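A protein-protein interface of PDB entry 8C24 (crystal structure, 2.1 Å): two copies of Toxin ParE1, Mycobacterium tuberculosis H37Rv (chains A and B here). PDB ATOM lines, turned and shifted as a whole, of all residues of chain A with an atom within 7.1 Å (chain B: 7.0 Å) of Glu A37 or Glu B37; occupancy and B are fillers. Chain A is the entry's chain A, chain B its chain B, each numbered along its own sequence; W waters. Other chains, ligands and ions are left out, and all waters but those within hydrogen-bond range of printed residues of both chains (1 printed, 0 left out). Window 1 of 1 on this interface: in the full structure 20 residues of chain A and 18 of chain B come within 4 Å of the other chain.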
ATOM      1  N   ALA A  31     -12.428 -21.786 -13.912  1.00  0.00           N
ATOM      2  CA  ALA A  31     -13.660 -22.330 -14.491  1.00  0.00           C
ATOM      3  C   ALA A  31     -14.885 -21.673 -13.866  1.00  0.00           C
ATOM      4  O   ALA A  31     -15.798 -21.220 -14.569  1.00  0.00           O
ATOM      5  CB  ALA A  31     -13.703 -23.848 -14.295  1.00  0.00           C
ATOM      6  N   GLU A  32     -14.884 -21.558 -12.541  1.00  0.00           N
ATOM      7  CA  GLU A  32     -16.024 -20.976 -11.838  1.00  0.00           C
ATOM      8  C   GLU A  32     -16.168 -19.501 -12.162  1.00  0.00           C
ATOM      9  O   GLU A  32     -17.275 -19.020 -12.431  1.00  0.00           O
ATOM     10  CB  GLU A  32     -15.859 -21.173 -10.327  1.00  0.00           C
ATOM     11  CG  GLU A  32     -17.090 -20.762  -9.508  1.00  0.00           C
ATOM     12  CD  GLU A  32     -17.032 -21.319  -8.099  1.00  0.00           C
ATOM     13  OE1 GLU A  32     -16.507 -20.613  -7.203  1.00  0.00           O
ATOM     14  OE2 GLU A  32     -17.486 -22.466  -7.894  1.00  0.00           O
ATOM     15  N   GLN A  33     -15.050 -18.761 -12.113  1.00  0.00           N
ATOM     16  CA  GLN A  33     -15.048 -17.339 -12.447  1.00  0.00           C
ATOM     17  C   GLN A  33     -15.633 -17.092 -13.834  1.00  0.00           C
ATOM     18  O   GLN A  33     -16.457 -16.187 -14.023  1.00  0.00           O
ATOM     19  CB  GLN A  33     -13.612 -16.790 -12.382  1.00  0.00           C
ATOM     20  CG  GLN A  33     -13.295 -16.058 -11.113  1.00  0.00           C
ATOM     21  CD  GLN A  33     -13.966 -14.701 -11.030  1.00  0.00           C
ATOM     22  OE1 GLN A  33     -14.914 -14.531 -10.270  1.00  0.00           O
ATOM     23  NE2 GLN A  33     -13.477 -13.726 -11.808  1.00  0.00           N
ATOM     24  N   TYR A  34     -15.199 -17.869 -14.830  1.00  0.00           N
ATOM     25  CA  TYR A  34     -15.695 -17.610 -16.179  1.00  0.00           C
ATOM     26  C   TYR A  34     -17.189 -17.890 -16.274  1.00  0.00           C
ATOM     27  O   TYR A  34     -17.929 -17.128 -16.909  1.00  0.00           O
ATOM     28  CB  TYR A  34     -14.927 -18.419 -17.235  1.00  0.00           C
ATOM     29  CG  TYR A  34     -15.350 -18.047 -18.658  1.00  0.00           C
ATOM     30  CD1 TYR A  34     -15.115 -16.767 -19.159  1.00  0.00           C
ATOM     31  CD2 TYR A  34     -16.005 -18.957 -19.489  1.00  0.00           C
ATOM     32  CE1 TYR A  34     -15.506 -16.398 -20.448  1.00  0.00           C
ATOM     33  CE2 TYR A  34     -16.408 -18.599 -20.797  1.00  0.00           C
ATOM     34  CZ  TYR A  34     -16.156 -17.319 -21.262  1.00  0.00           C
ATOM     35  OH  TYR A  34     -16.540 -16.952 -22.543  1.00  0.00           O
ATOM     36  N   LEU A  35     -17.648 -18.959 -15.630  1.00  0.00           N
ATOM     37  CA  LEU A  35     -19.093 -19.275 -15.682  1.00  0.00           C
ATOM     38  C   LEU A  35     -19.862 -18.160 -14.975  1.00  0.00           C
ATOM     39  O   LEU A  35     -20.936 -17.822 -15.445  1.00  0.00           O
ATOM     40  CB  LEU A  35     -19.349 -20.657 -15.084  1.00  0.00           C
ATOM     41  CG  LEU A  35     -19.388 -21.812 -16.082  1.00  0.00           C
ATOM     42  CD1 LEU A  35     -20.445 -21.604 -17.143  1.00  0.00           C
ATOM     43  CD2 LEU A  35     -18.042 -22.006 -16.728  1.00  0.00           C
ATOM     44  N   ARG A  36     -19.279 -17.592 -13.919  1.00  0.00           N
ATOM     45  CA  ARG A  36     -19.916 -16.477 -13.179  1.00  0.00           C
ATOM     46  C   ARG A  36     -20.019 -15.285 -14.124  1.00  0.00           C
ATOM     47  O   ARG A  36     -21.024 -14.591 -14.061  1.00  0.00           O
ATOM     48  CB  ARG A  36     -19.095 -16.059 -11.961  1.00  0.00           C
ATOM     49  CG  ARG A  36     -19.301 -16.924 -10.733  1.00  0.00           C
ATOM     50  CD  ARG A  36     -20.694 -16.838 -10.171  1.00  0.00           C
ATOM     51  NE  ARG A  36     -20.782 -17.754  -9.060  1.00  0.00           N
ATOM     52  CZ  ARG A  36     -21.897 -18.120  -8.465  1.00  0.00           C
ATOM     53  NH1 ARG A  36     -23.054 -17.630  -8.849  1.00  0.00           N
ATOM     54  NH2 ARG A  36     -21.852 -18.966  -7.464  1.00  0.00           N
ATOM     55  N   GLU A  37     -19.002 -15.097 -14.964  1.00  0.00           N
ATOM     56  CA  GLU A  37     -19.014 -13.998 -15.925  1.00  0.00           C
ATOM     57  C   GLU A  37     -20.133 -14.174 -16.943  1.00  0.00           C
ATOM     58  O   GLU A  37     -20.829 -13.210 -17.278  1.00  0.00           O
ATOM     59  CB  GLU A  37     -17.653 -13.885 -16.617  1.00  0.00           C
ATOM     60  CG  GLU A  37     -17.344 -12.488 -17.153  1.00  0.00           C
ATOM     61  CD  GLU A  37     -16.012 -12.429 -17.863  1.00  0.00           C
ATOM     62  OE1 GLU A  37     -14.998 -12.820 -17.247  1.00  0.00           O
ATOM     63  OE2 GLU A  37     -15.980 -12.013 -19.042  1.00  0.00           O
ATOM     64  N   LEU A  38     -20.345 -15.404 -17.428  1.00  0.00           N
ATOM     65  CA  LEU A  38     -21.480 -15.659 -18.319  1.00  0.00           C
ATOM     66  C   LEU A  38     -22.807 -15.479 -17.587  1.00  0.00           C
ATOM     67  O   LEU A  38     -23.785 -14.980 -18.170  1.00  0.00           O
ATOM     68  CB  LEU A  38     -21.397 -17.073 -18.908  1.00  0.00           C
ATOM     69  CG  LEU A  38     -20.207 -17.389 -19.837  1.00  0.00           C
ATOM     70  CD1 LEU A  38     -20.344 -18.749 -20.471  1.00  0.00           C
ATOM     71  CD2 LEU A  38     -20.050 -16.339 -20.917  1.00  0.00           C
ATOM     72  N   GLN A  39     -22.867 -15.903 -16.310  1.00  0.00           N
ATOM     73  CA  GLN A  39     -24.090 -15.724 -15.532  1.00  0.00           C
ATOM     74  C   GLN A  39     -24.482 -14.251 -15.429  1.00  0.00           C
ATOM     75  O   GLN A  39     -25.673 -13.920 -15.481  1.00  0.00           O
ATOM     76  CB  GLN A  39     -23.922 -16.336 -14.134  1.00  0.00           C
ATOM     77  CG  GLN A  39     -25.163 -16.244 -13.273  1.00  0.00           C
ATOM     78  CD  GLN A  39     -24.891 -16.652 -11.822  1.00  0.00           C
ATOM     79  OE1 GLN A  39     -23.740 -16.741 -11.402  1.00  0.00           O
ATOM     80  NE2 GLN A  39     -25.955 -16.900 -11.062  1.00  0.00           N
ATOM     81  N   HIS A  40     -23.490 -13.358 -15.277  1.00  0.00           N
ATOM     82  CA  HIS A  40     -23.747 -11.918 -15.197  1.00  0.00           C
ATOM     83  C   HIS A  40     -24.472 -11.413 -16.439  1.00  0.00           C
ATOM     84  O   HIS A  40     -25.412 -10.617 -16.347  1.00  0.00           O
ATOM     85  CB  HIS A  40     -22.425 -11.145 -15.029  1.00  0.00           C
ATOM     86  CG  HIS A  40     -21.975 -10.999 -13.609  1.00  0.00           C
ATOM     87  ND1 HIS A  40     -22.352  -9.937 -12.811  1.00  0.00           N
ATOM     88  CD2 HIS A  40     -21.175 -11.779 -12.842  1.00  0.00           C
ATOM     89  CE1 HIS A  40     -21.811 -10.073 -11.613  1.00  0.00           C
ATOM     90  NE2 HIS A  40     -21.095 -11.184 -11.604  1.00  0.00           N
ATOM     91  N   ALA A  41     -24.014 -11.828 -17.620  1.00  0.00           N
ATOM     92  CA  ALA A  41     -24.673 -11.377 -18.837  1.00  0.00           C
ATOM     93  C   ALA A  41     -26.071 -11.976 -18.947  1.00  0.00           C
ATOM     94  O   ALA A  41     -27.017 -11.292 -19.353  1.00  0.00           O
ATOM     95  CB  ALA A  41     -23.820 -11.719 -20.062  1.00  0.00           C
ATOM     96  N   ILE A  42     -26.233 -13.240 -18.558  1.00  0.00           N
ATOM     97  CA  ILE A  42     -27.577 -13.824 -18.580  1.00  0.00           C
ATOM     98  C   ILE A  42     -28.498 -13.058 -17.637  1.00  0.00           C
ATOM     99  O   ILE A  42     -29.619 -12.700 -18.008  1.00  0.00           O
ATOM    100  CB  ILE A  42     -27.529 -15.325 -18.239  1.00  0.00           C
ATOM    101  CG1 ILE A  42     -26.877 -16.114 -19.379  1.00  0.00           C
ATOM    102  CG2 ILE A  42     -28.931 -15.866 -17.961  1.00  0.00           C
ATOM    103  CD1 ILE A  42     -26.149 -17.361 -18.872  1.00  0.00           C
ATOM    104  N   ARG A  44     -28.228  -9.928 -16.700  1.00  0.00           N
ATOM    105  CA  ARG A  44     -28.496  -8.613 -17.271  1.00  0.00           C
ATOM    106  C   ARG A  44     -29.598  -8.693 -18.313  1.00  0.00           C
ATOM    107  O   ARG A  44     -30.529  -7.885 -18.310  1.00  0.00           O
ATOM    108  CB  ARG A  44     -27.222  -8.034 -17.893  1.00  0.00           C
ATOM    109  CG  ARG A  44     -26.547  -6.962 -17.063  1.00  0.00           C
ATOM    110  CD  ARG A  44     -25.478  -6.233 -17.883  1.00  0.00           C
ATOM    111  NE  ARG A  44     -24.637  -7.176 -18.619  1.00  0.00           N
ATOM    112  CZ  ARG A  44     -24.311  -7.047 -19.899  1.00  0.00           C
ATOM    113  NH1 ARG A  44     -24.742  -5.995 -20.588  1.00  0.00           N
ATOM    114  NH2 ARG A  44     -23.539  -7.959 -20.488  1.00  0.00           N
ATOM    115  N   LEU A  65     -26.482 -11.145 -27.367  1.00  0.00           N
ATOM    116  CA  LEU A  65     -25.746 -10.345 -26.397  1.00  0.00           C
ATOM    117  C   LEU A  65     -24.385 -10.989 -26.203  1.00  0.00           C
ATOM    118  O   LEU A  65     -24.310 -12.143 -25.782  1.00  0.00           O
ATOM    119  CB  LEU A  65     -26.512 -10.251 -25.067  1.00  0.00           C
ATOM    120  CG  LEU A  65     -25.762  -9.516 -23.945  1.00  0.00           C
ATOM    121  CD1 LEU A  65     -25.680  -8.039 -24.281  1.00  0.00           C
ATOM    122  CD2 LEU A  65     -26.450  -9.728 -22.601  1.00  0.00           C
ATOM    123  N   SER A  66     -23.314 -10.264 -26.523  1.00  0.00           N
ATOM    124  CA  SER A  66     -21.978 -10.818 -26.352  1.00  0.00           C
ATOM    125  C   SER A  66     -21.647 -10.969 -24.870  1.00  0.00           C
ATOM    126  O   SER A  66     -22.088 -10.180 -24.038  1.00  0.00           O
ATOM    127  CB  SER A  66     -20.944  -9.921 -27.026  1.00  0.00           C
ATOM    128  OG  SER A  66     -21.363  -9.546 -28.328  1.00  0.00           O
ATOM    129  N   ALA A  67     -20.855 -11.992 -24.540  1.00  0.00           N
ATOM    130  CA  ALA A  67     -20.511 -12.258 -23.144  1.00  0.00           C
ATOM    131  C   ALA A  67     -19.223 -13.066 -23.064  1.00  0.00           C
ATOM    132  O   ALA A  67     -19.197 -14.222 -23.485  1.00  0.00           O
ATOM    133  CB  ALA A  67     -21.651 -13.002 -22.446  1.00  0.00           C
ATOM    134  N   GLY A  68     -18.183 -12.499 -22.459  1.00  0.00           N
ATOM    135  CA  GLY A  68     -16.898 -13.190 -22.423  1.00  0.00           C
ATOM    136  C   GLY A  68     -16.465 -13.475 -23.849  1.00  0.00           C
ATOM    137  O   GLY A  68     -16.502 -12.594 -24.714  1.00  0.00           O
ATOM    138  N   SER A  69     -16.115 -14.732 -24.118  1.00  0.00           N
ATOM    139  CA  SER A  69     -15.774 -15.194 -25.456  1.00  0.00           C
ATOM    140  C   SER A  69     -16.979 -15.745 -26.231  1.00  0.00           C
ATOM    141  O   SER A  69     -16.797 -16.301 -27.314  1.00  0.00           O
ATOM    142  CB  SER A  69     -14.694 -16.274 -25.359  1.00  0.00           C
ATOM    143  OG  SER A  69     -13.423 -15.714 -25.080  1.00  0.00           O
ATOM    144  N   GLU B  32     -24.363  -0.950 -12.994  1.00  0.00           N
ATOM    145  CA  GLU B  32     -23.474  -1.570 -12.020  1.00  0.00           C
ATOM    146  C   GLU B  32     -23.136  -3.001 -12.406  1.00  0.00           C
ATOM    147  O   GLU B  32     -22.004  -3.456 -12.201  1.00  0.00           O
ATOM    148  CB  GLU B  32     -24.123  -1.539 -10.634  1.00  0.00           C
ATOM    149  CG  GLU B  32     -23.203  -1.998  -9.506  1.00  0.00           C
ATOM    150  CD  GLU B  32     -23.804  -1.751  -8.133  1.00  0.00           C
ATOM    151  OE1 GLU B  32     -25.044  -1.652  -8.038  1.00  0.00           O
ATOM    152  OE2 GLU B  32     -23.039  -1.668  -7.153  1.00  0.00           O
ATOM    153  N   GLN B  33     -24.113  -3.739 -12.936  1.00  0.00           N
ATOM    154  CA  GLN B  33     -23.861  -5.144 -13.228  1.00  0.00           C
ATOM    155  C   GLN B  33     -22.916  -5.293 -14.412  1.00  0.00           C
ATOM    156  O   GLN B  33     -22.029  -6.153 -14.393  1.00  0.00           O
ATOM    157  CB  GLN B  33     -25.172  -5.906 -13.474  1.00  0.00           C
ATOM    158  CG  GLN B  33     -24.868  -7.405 -13.629  1.00  0.00           C
ATOM    159  CD  GLN B  33     -26.081  -8.318 -13.713  1.00  0.00           C
ATOM    160  OE1 GLN B  33     -27.217  -7.849 -13.564  1.00  0.00           O
ATOM    161  NE2 GLN B  33     -25.861  -9.606 -14.026  1.00  0.00           N
ATOM    162  N   TYR B  34     -23.063  -4.446 -15.433  1.00  0.00           N
ATOM    163  CA  TYR B  34     -22.148  -4.518 -16.561  1.00  0.00           C
ATOM    164  C   TYR B  34     -20.720  -4.175 -16.142  1.00  0.00           C
ATOM    165  O   TYR B  34     -19.762  -4.778 -16.640  1.00  0.00           O
ATOM    166  CB  TYR B  34     -22.599  -3.605 -17.698  1.00  0.00           C
ATOM    167  CG  TYR B  34     -21.754  -3.852 -18.928  1.00  0.00           C
ATOM    168  CD1 TYR B  34     -21.803  -5.080 -19.582  1.00  0.00           C
ATOM    169  CD2 TYR B  34     -20.875  -2.885 -19.414  1.00  0.00           C
ATOM    170  CE1 TYR B  34     -21.025  -5.336 -20.705  1.00  0.00           C
ATOM    171  CE2 TYR B  34     -20.085  -3.134 -20.537  1.00  0.00           C
ATOM    172  CZ  TYR B  34     -20.169  -4.365 -21.181  1.00  0.00           C
ATOM    173  OH  TYR B  34     -19.394  -4.636 -22.297  1.00  0.00           O
ATOM    174  N   LEU B  35     -20.546  -3.213 -15.223  1.00  0.00           N
ATOM    175  CA  LEU B  35     -19.184  -2.923 -14.784  1.00  0.00           C
ATOM    176  C   LEU B  35     -18.630  -4.087 -13.972  1.00  0.00           C
ATOM    177  O   LEU B  35     -17.434  -4.411 -14.070  1.00  0.00           O
ATOM    178  CB  LEU B  35     -19.136  -1.606 -14.002  1.00  0.00           C
ATOM    179  CG  LEU B  35     -18.708  -0.346 -14.779  1.00  0.00           C
ATOM    180  CD1 LEU B  35     -17.319  -0.504 -15.397  1.00  0.00           C
ATOM    181  CD2 LEU B  35     -19.706   0.003 -15.860  1.00  0.00           C
ATOM    182  N   ARG B  36     -19.501  -4.761 -13.199  1.00  0.00           N
ATOM    183  CA  ARG B  36     -19.082  -5.955 -12.468  1.00  0.00           C
ATOM    184  C   ARG B  36     -18.698  -7.080 -13.426  1.00  0.00           C
ATOM    185  O   ARG B  36     -17.736  -7.815 -13.179  1.00  0.00           O
ATOM    186  CB  ARG B  36     -20.201  -6.422 -11.531  1.00  0.00           C
ATOM    187  CG  ARG B  36     -20.464  -5.502 -10.339  1.00  0.00           C
ATOM    188  CD  ARG B  36     -19.391  -5.659  -9.282  1.00  0.00           C
ATOM    189  NE  ARG B  36     -19.736  -4.953  -8.058  1.00  0.00           N
ATOM    190  CZ  ARG B  36     -18.857  -4.467  -7.185  1.00  0.00           C
ATOM    191  NH1 ARG B  36     -17.550  -4.609  -7.389  1.00  0.00           N
ATOM    192  NH2 ARG B  36     -19.295  -3.843  -6.092  1.00  0.00           N
ATOM    193  N   GLU B  37     -19.460  -7.252 -14.508  1.00  0.00           N
ATOM    194  CA  GLU B  37     -19.073  -8.209 -15.544  1.00  0.00           C
ATOM    195  C   GLU B  37     -17.665  -7.914 -16.061  1.00  0.00           C
ATOM    196  O   GLU B  37     -16.800  -8.797 -16.078  1.00  0.00           O
ATOM    197  CB  GLU B  37     -20.092  -8.188 -16.687  1.00  0.00           C
ATOM    198  CG  GLU B  37     -20.082  -9.445 -17.534  1.00  0.00           C
ATOM    199  CD  GLU B  37     -21.137  -9.422 -18.646  1.00  0.00           C
ATOM    200  OE1 GLU B  37     -22.270  -8.929 -18.418  1.00  0.00           O
ATOM    201  OE2 GLU B  37     -20.835  -9.902 -19.760  1.00  0.00           O
ATOM    202  N   LEU B  38     -17.406  -6.666 -16.458  1.00  0.00           N
ATOM    203  CA  LEU B  38     -16.043  -6.273 -16.848  1.00  0.00           C
ATOM    204  C   LEU B  38     -15.024  -6.543 -15.733  1.00  0.00           C
ATOM    205  O   LEU B  38     -13.891  -6.963 -16.000  1.00  0.00           O
ATOM    206  CB  LEU B  38     -16.017  -4.795 -17.226  1.00  0.00           C
ATOM    207  CG  LEU B  38     -16.668  -4.424 -18.560  1.00  0.00           C
ATOM    208  CD1 LEU B  38     -16.438  -2.938 -18.821  1.00  0.00           C
ATOM    209  CD2 LEU B  38     -16.115  -5.281 -19.720  1.00  0.00           C
ATOM    210  N   GLN B  39     -15.411  -6.323 -14.473  1.00  0.00           N
ATOM    211  CA  GLN B  39     -14.490  -6.600 -13.368  1.00  0.00           C
ATOM    212  C   GLN B  39     -14.138  -8.087 -13.269  1.00  0.00           C
ATOM    213  O   GLN B  39     -12.991  -8.436 -12.972  1.00  0.00           O
ATOM    214  CB  GLN B  39     -15.084  -6.106 -12.051  1.00  0.00           C
ATOM    215  CG  GLN B  39     -14.197  -6.385 -10.867  1.00  0.00           C
ATOM    216  CD  GLN B  39     -14.860  -6.030  -9.564  1.00  0.00           C
ATOM    217  OE1 GLN B  39     -16.065  -5.794  -9.513  1.00  0.00           O
ATOM    218  NE2 GLN B  39     -14.075  -5.972  -8.503  1.00  0.00           N
ATOM    219  N   HIS B  40     -15.112  -8.983 -13.491  1.00  0.00           N
ATOM    220  CA  HIS B  40     -14.809 -10.414 -13.516  1.00  0.00           C
ATOM    221  C   HIS B  40     -13.759 -10.754 -14.568  1.00  0.00           C
ATOM    222  O   HIS B  40     -12.879 -11.591 -14.336  1.00  0.00           O
ATOM    223  CB  HIS B  40     -16.076 -11.230 -13.807  1.00  0.00           C
ATOM    224  CG  HIS B  40     -16.877 -11.550 -12.596  1.00  0.00           C
ATOM    225  ND1 HIS B  40     -17.188 -12.843 -12.230  1.00  0.00           N
ATOM    226  CD2 HIS B  40     -17.419 -10.746 -11.651  1.00  0.00           C
ATOM    227  CE1 HIS B  40     -17.894 -12.821 -11.114  1.00  0.00           C
ATOM    228  NE2 HIS B  40     -18.045 -11.562 -10.739  1.00  0.00           N
ATOM    229  N   ALA B  41     -13.878 -10.178 -15.758  1.00  0.00           N
ATOM    230  CA  ALA B  41     -12.875 -10.437 -16.787  1.00  0.00           C
ATOM    231  C   ALA B  41     -11.511  -9.881 -16.378  1.00  0.00           C
ATOM    232  O   ALA B  41     -10.480 -10.548 -16.551  1.00  0.00           O
ATOM    233  CB  ALA B  41     -13.345  -9.849 -18.117  1.00  0.00           C
ATOM    234  N   ILE B  42     -11.478  -8.673 -15.818  1.00  0.00           N
ATOM    235  CA  ILE B  42     -10.207  -8.125 -15.326  1.00  0.00           C
ATOM    236  C   ILE B  42      -9.616  -9.036 -14.254  1.00  0.00           C
ATOM    237  O   ILE B  42      -8.425  -9.368 -14.290  1.00  0.00           O
ATOM    238  CB  ILE B  42     -10.399  -6.682 -14.818  1.00  0.00           C
ATOM    239  CG1 ILE B  42     -10.702  -5.759 -16.011  1.00  0.00           C
ATOM    240  CG2 ILE B  42      -9.143  -6.181 -14.029  1.00  0.00           C
ATOM    241  CD1 ILE B  42     -11.210  -4.374 -15.605  1.00  0.00           C
ATOM    242  N   ASP B  43     -10.448  -9.503 -13.320  1.00  0.00           N
ATOM    243  CA  ASP B  43      -9.955 -10.403 -12.282  1.00  0.00           C
ATOM    244  C   ASP B  43      -9.449 -11.713 -12.871  1.00  0.00           C
ATOM    245  O   ASP B  43      -8.451 -12.266 -12.394  1.00  0.00           O
ATOM    246  CB  ASP B  43     -11.059 -10.672 -11.260  1.00  0.00           C
ATOM    247  CG  ASP B  43     -11.195  -9.557 -10.239  1.00  0.00           C
ATOM    248  OD1 ASP B  43     -10.224  -8.786 -10.040  1.00  0.00           O
ATOM    249  OD2 ASP B  43     -12.284  -9.445  -9.640  1.00  0.00           O
ATOM    250  N   ARG B  44     -10.138 -12.238 -13.891  1.00  0.00           N
ATOM    251  CA  ARG B  44      -9.691 -13.461 -14.553  1.00  0.00           C
ATOM    252  C   ARG B  44      -8.273 -13.304 -15.082  1.00  0.00           C
ATOM    253  O   ARG B  44      -7.398 -14.132 -14.811  1.00  0.00           O
ATOM    254  CB  ARG B  44     -10.630 -13.803 -15.707  1.00  0.00           C
ATOM    255  CG  ARG B  44     -11.679 -14.852 -15.448  1.00  0.00           C
ATOM    256  CD  ARG B  44     -12.683 -14.841 -16.602  1.00  0.00           C
ATOM    257  NE  ARG B  44     -12.092 -15.284 -17.866  1.00  0.00           N
ATOM    258  CZ  ARG B  44     -12.379 -14.785 -19.070  1.00  0.00           C
ATOM    259  NH1 ARG B  44     -13.262 -13.796 -19.223  1.00  0.00           N
ATOM    260  NH2 ARG B  44     -11.780 -15.285 -20.142  1.00  0.00           N
ATOM    261  N   LEU B  65      -8.105 -10.056 -24.153  1.00  0.00           N
ATOM    262  CA  LEU B  65      -9.090 -10.955 -23.566  1.00  0.00           C
ATOM    263  C   LEU B  65     -10.472 -10.400 -23.852  1.00  0.00           C
ATOM    264  O   LEU B  65     -10.782  -9.265 -23.466  1.00  0.00           O
ATOM    265  CB  LEU B  65      -8.878 -11.124 -22.052  1.00  0.00           C
ATOM    266  CG  LEU B  65      -9.856 -12.066 -21.317  1.00  0.00           C
ATOM    267  CD1 LEU B  65      -9.564 -13.542 -21.633  1.00  0.00           C
ATOM    268  CD2 LEU B  65      -9.863 -11.840 -19.798  1.00  0.00           C
ATOM    269  N   SER B  66     -11.299 -11.206 -24.514  1.00  0.00           N
ATOM    270  CA  SER B  66     -12.657 -10.800 -24.809  1.00  0.00           C
ATOM    271  C   SER B  66     -13.442 -10.694 -23.518  1.00  0.00           C
ATOM    272  O   SER B  66     -13.388 -11.583 -22.660  1.00  0.00           O
ATOM    273  CB  SER B  66     -13.324 -11.792 -25.756  1.00  0.00           C
ATOM    274  OG  SER B  66     -12.995 -11.468 -27.090  1.00  0.00           O
ATOM    275  N   ALA B  67     -14.173  -9.602 -23.385  1.00  0.00           N
ATOM    276  CA  ALA B  67     -14.903  -9.303 -22.178  1.00  0.00           C
ATOM    277  C   ALA B  67     -16.296  -8.861 -22.613  1.00  0.00           C
ATOM    278  O   ALA B  67     -16.693  -7.710 -22.446  1.00  0.00           O
ATOM    279  CB  ALA B  67     -14.173  -8.238 -21.363  1.00  0.00           C
ATOM    280  N   GLY B  68     -17.009  -9.794 -23.248  1.00  0.00           N
ATOM    281  CA  GLY B  68     -18.329  -9.514 -23.796  1.00  0.00           C
ATOM    282  C   GLY B  68     -18.204  -8.523 -24.921  1.00  0.00           C
ATOM    283  O   GLY B  68     -17.443  -8.724 -25.888  1.00  0.00           O
ATOM    284  N   SER B  69     -18.915  -7.406 -24.802  1.00  0.00           N
ATOM    285  CA  SER B  69     -18.940  -6.508 -25.944  1.00  0.00           C
ATOM    286  C   SER B  69     -17.727  -5.585 -25.988  1.00  0.00           C
ATOM    287  O   SER B  69     -17.625  -4.779 -26.918  1.00  0.00           O
ATOM    288  CB  SER B  69     -20.253  -5.715 -25.959  1.00  0.00           C
ATOM    289  OG  SER B  69     -20.094  -4.432 -25.410  1.00  0.00           O
HETATM  290  O   HOH W   1     -12.750 -14.460 -22.610  1.00  0.00           O
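NH1 of Arg B44 is in salt-bridge range of OE1 of Glu A37. The backbone carbonyl oxygen (O) of His A40 lies within hydrogen-bond range of the side-chain amide nitrogen (NE2) of Gln B33. NE2 of His B40 sits at hydrogen-bond distance from NE2 of His A40, 3.2 Å away. The side-chain carboxylate (OE1) of Glu B37 lies within salt-bridge range of the guanidinium group (NH2) of Arg A44 (2.6 Å). OE1 of Glu B37 sits close to N of Ala A41, 3.5 Å away. O of His B40 sits at hydrogen-bond distance from NE2 of Gln A33. OE1 of Glu A37 sits close to N of Ala B41 (3.2 Å). The backbone carbonyl oxygen of Gly A68 is in hydrogen-bond range of the backbone NH of Gly B68 (3.2 Å).
The side-chain amide oxygen of Gln A39 lies within hydrogen-bond range of the guanidinium group of Arg A36 (2.8 Å). OG of Ser B69 sits at hydrogen-bond distance from OH of Tyr B34 (3.2 Å). The backbone NH (N) of Ser A69 lies within hydrogen-bond range of the side-chain hydroxyl (OH) of Tyr A34 (2.8 Å). The guanidinium group (NH1) of Arg B36 sits at hydrogen-bond distance from the side-chain amide oxygen (OE1) of Gln B39, at 2.8 Å.
Gln A33 touches Asp B43 (NE2 to CB, 3.9 Å). Glu A37 touches Glu B37 (O to CG, 3.8 Å). Glu A37 touches His B40 (OE1 to C, 3.6 Å). CB of Arg B36 touches CE1 of His A40 (3.99 Å). Glu B37 touches His A40. Arg A44 touches Gln B33. CB of Ser A66 touches N of Ser B69 (3.9 Å). Ala A67 touches Gly B68. Gly A68 touches Ser B66. Ser A69 touches Ser B66 (OG to CB, 3.98 Å).
Of chain B, only Glu B37, His B40, Ala B41 and Arg B44 come within 4 Å of Glu A37. Of the printed residues of chain B, Gly A68 touches Ser B66 and Gly B68. Of the printed residues of chain A, Tyr B34 touches Arg A44 (3.2 Å). Glu B37 touches just these residues of chain A: Glu A37 (3.8 Å), His A40 (3.8 Å), Ala A41 (3.5 Å) and Arg A44 (2.6 Å). Printed residues of chain A within 4 Å of Ala B41: Glu A37. Printed residues of chain A within 4 Å of Arg B44: Tyr A34 (3.4 Å) and Glu A37 (2.8 Å).
Printed residues of chain B that touch a printed residue of chain A: Gln B33, Tyr B34, Arg B36, Glu B37, His B40, Ala B41, Asp B43, Arg B44, Ser B66, Gly B68 and Ser B69. Hydrophobic or aromatic side chains of chain B that line the printed part of chain A: Tyr B34, His B40 and Ala B41. Among the printed residues, 22 pairs touch across the chains. Among the printed residues, Asp or Glu carboxylates within 4 Å of a Lys or Arg side-chain nitrogen of the other chain: Glu A37 with Arg B44 (2.8 Å) and Arg A44 with Glu B37 (2.6 Å).
Tyr A34 touches Arg B44, and with the chains exchanged Arg A44 touches Tyr B34. Glu A37 touches His B40, and with the chains exchanged His A40 touches Glu B37. Glu A37 touches Ala B41, and with the chains exchanged Ala A41 touches Glu B37. His A40 touches its own counterpart, His B40. 17 positions are printed for both chains.
Water W1 lies within hydrogen-bond range of NH2 of Arg B44, OG of Ser A69 and O of Ser B66.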
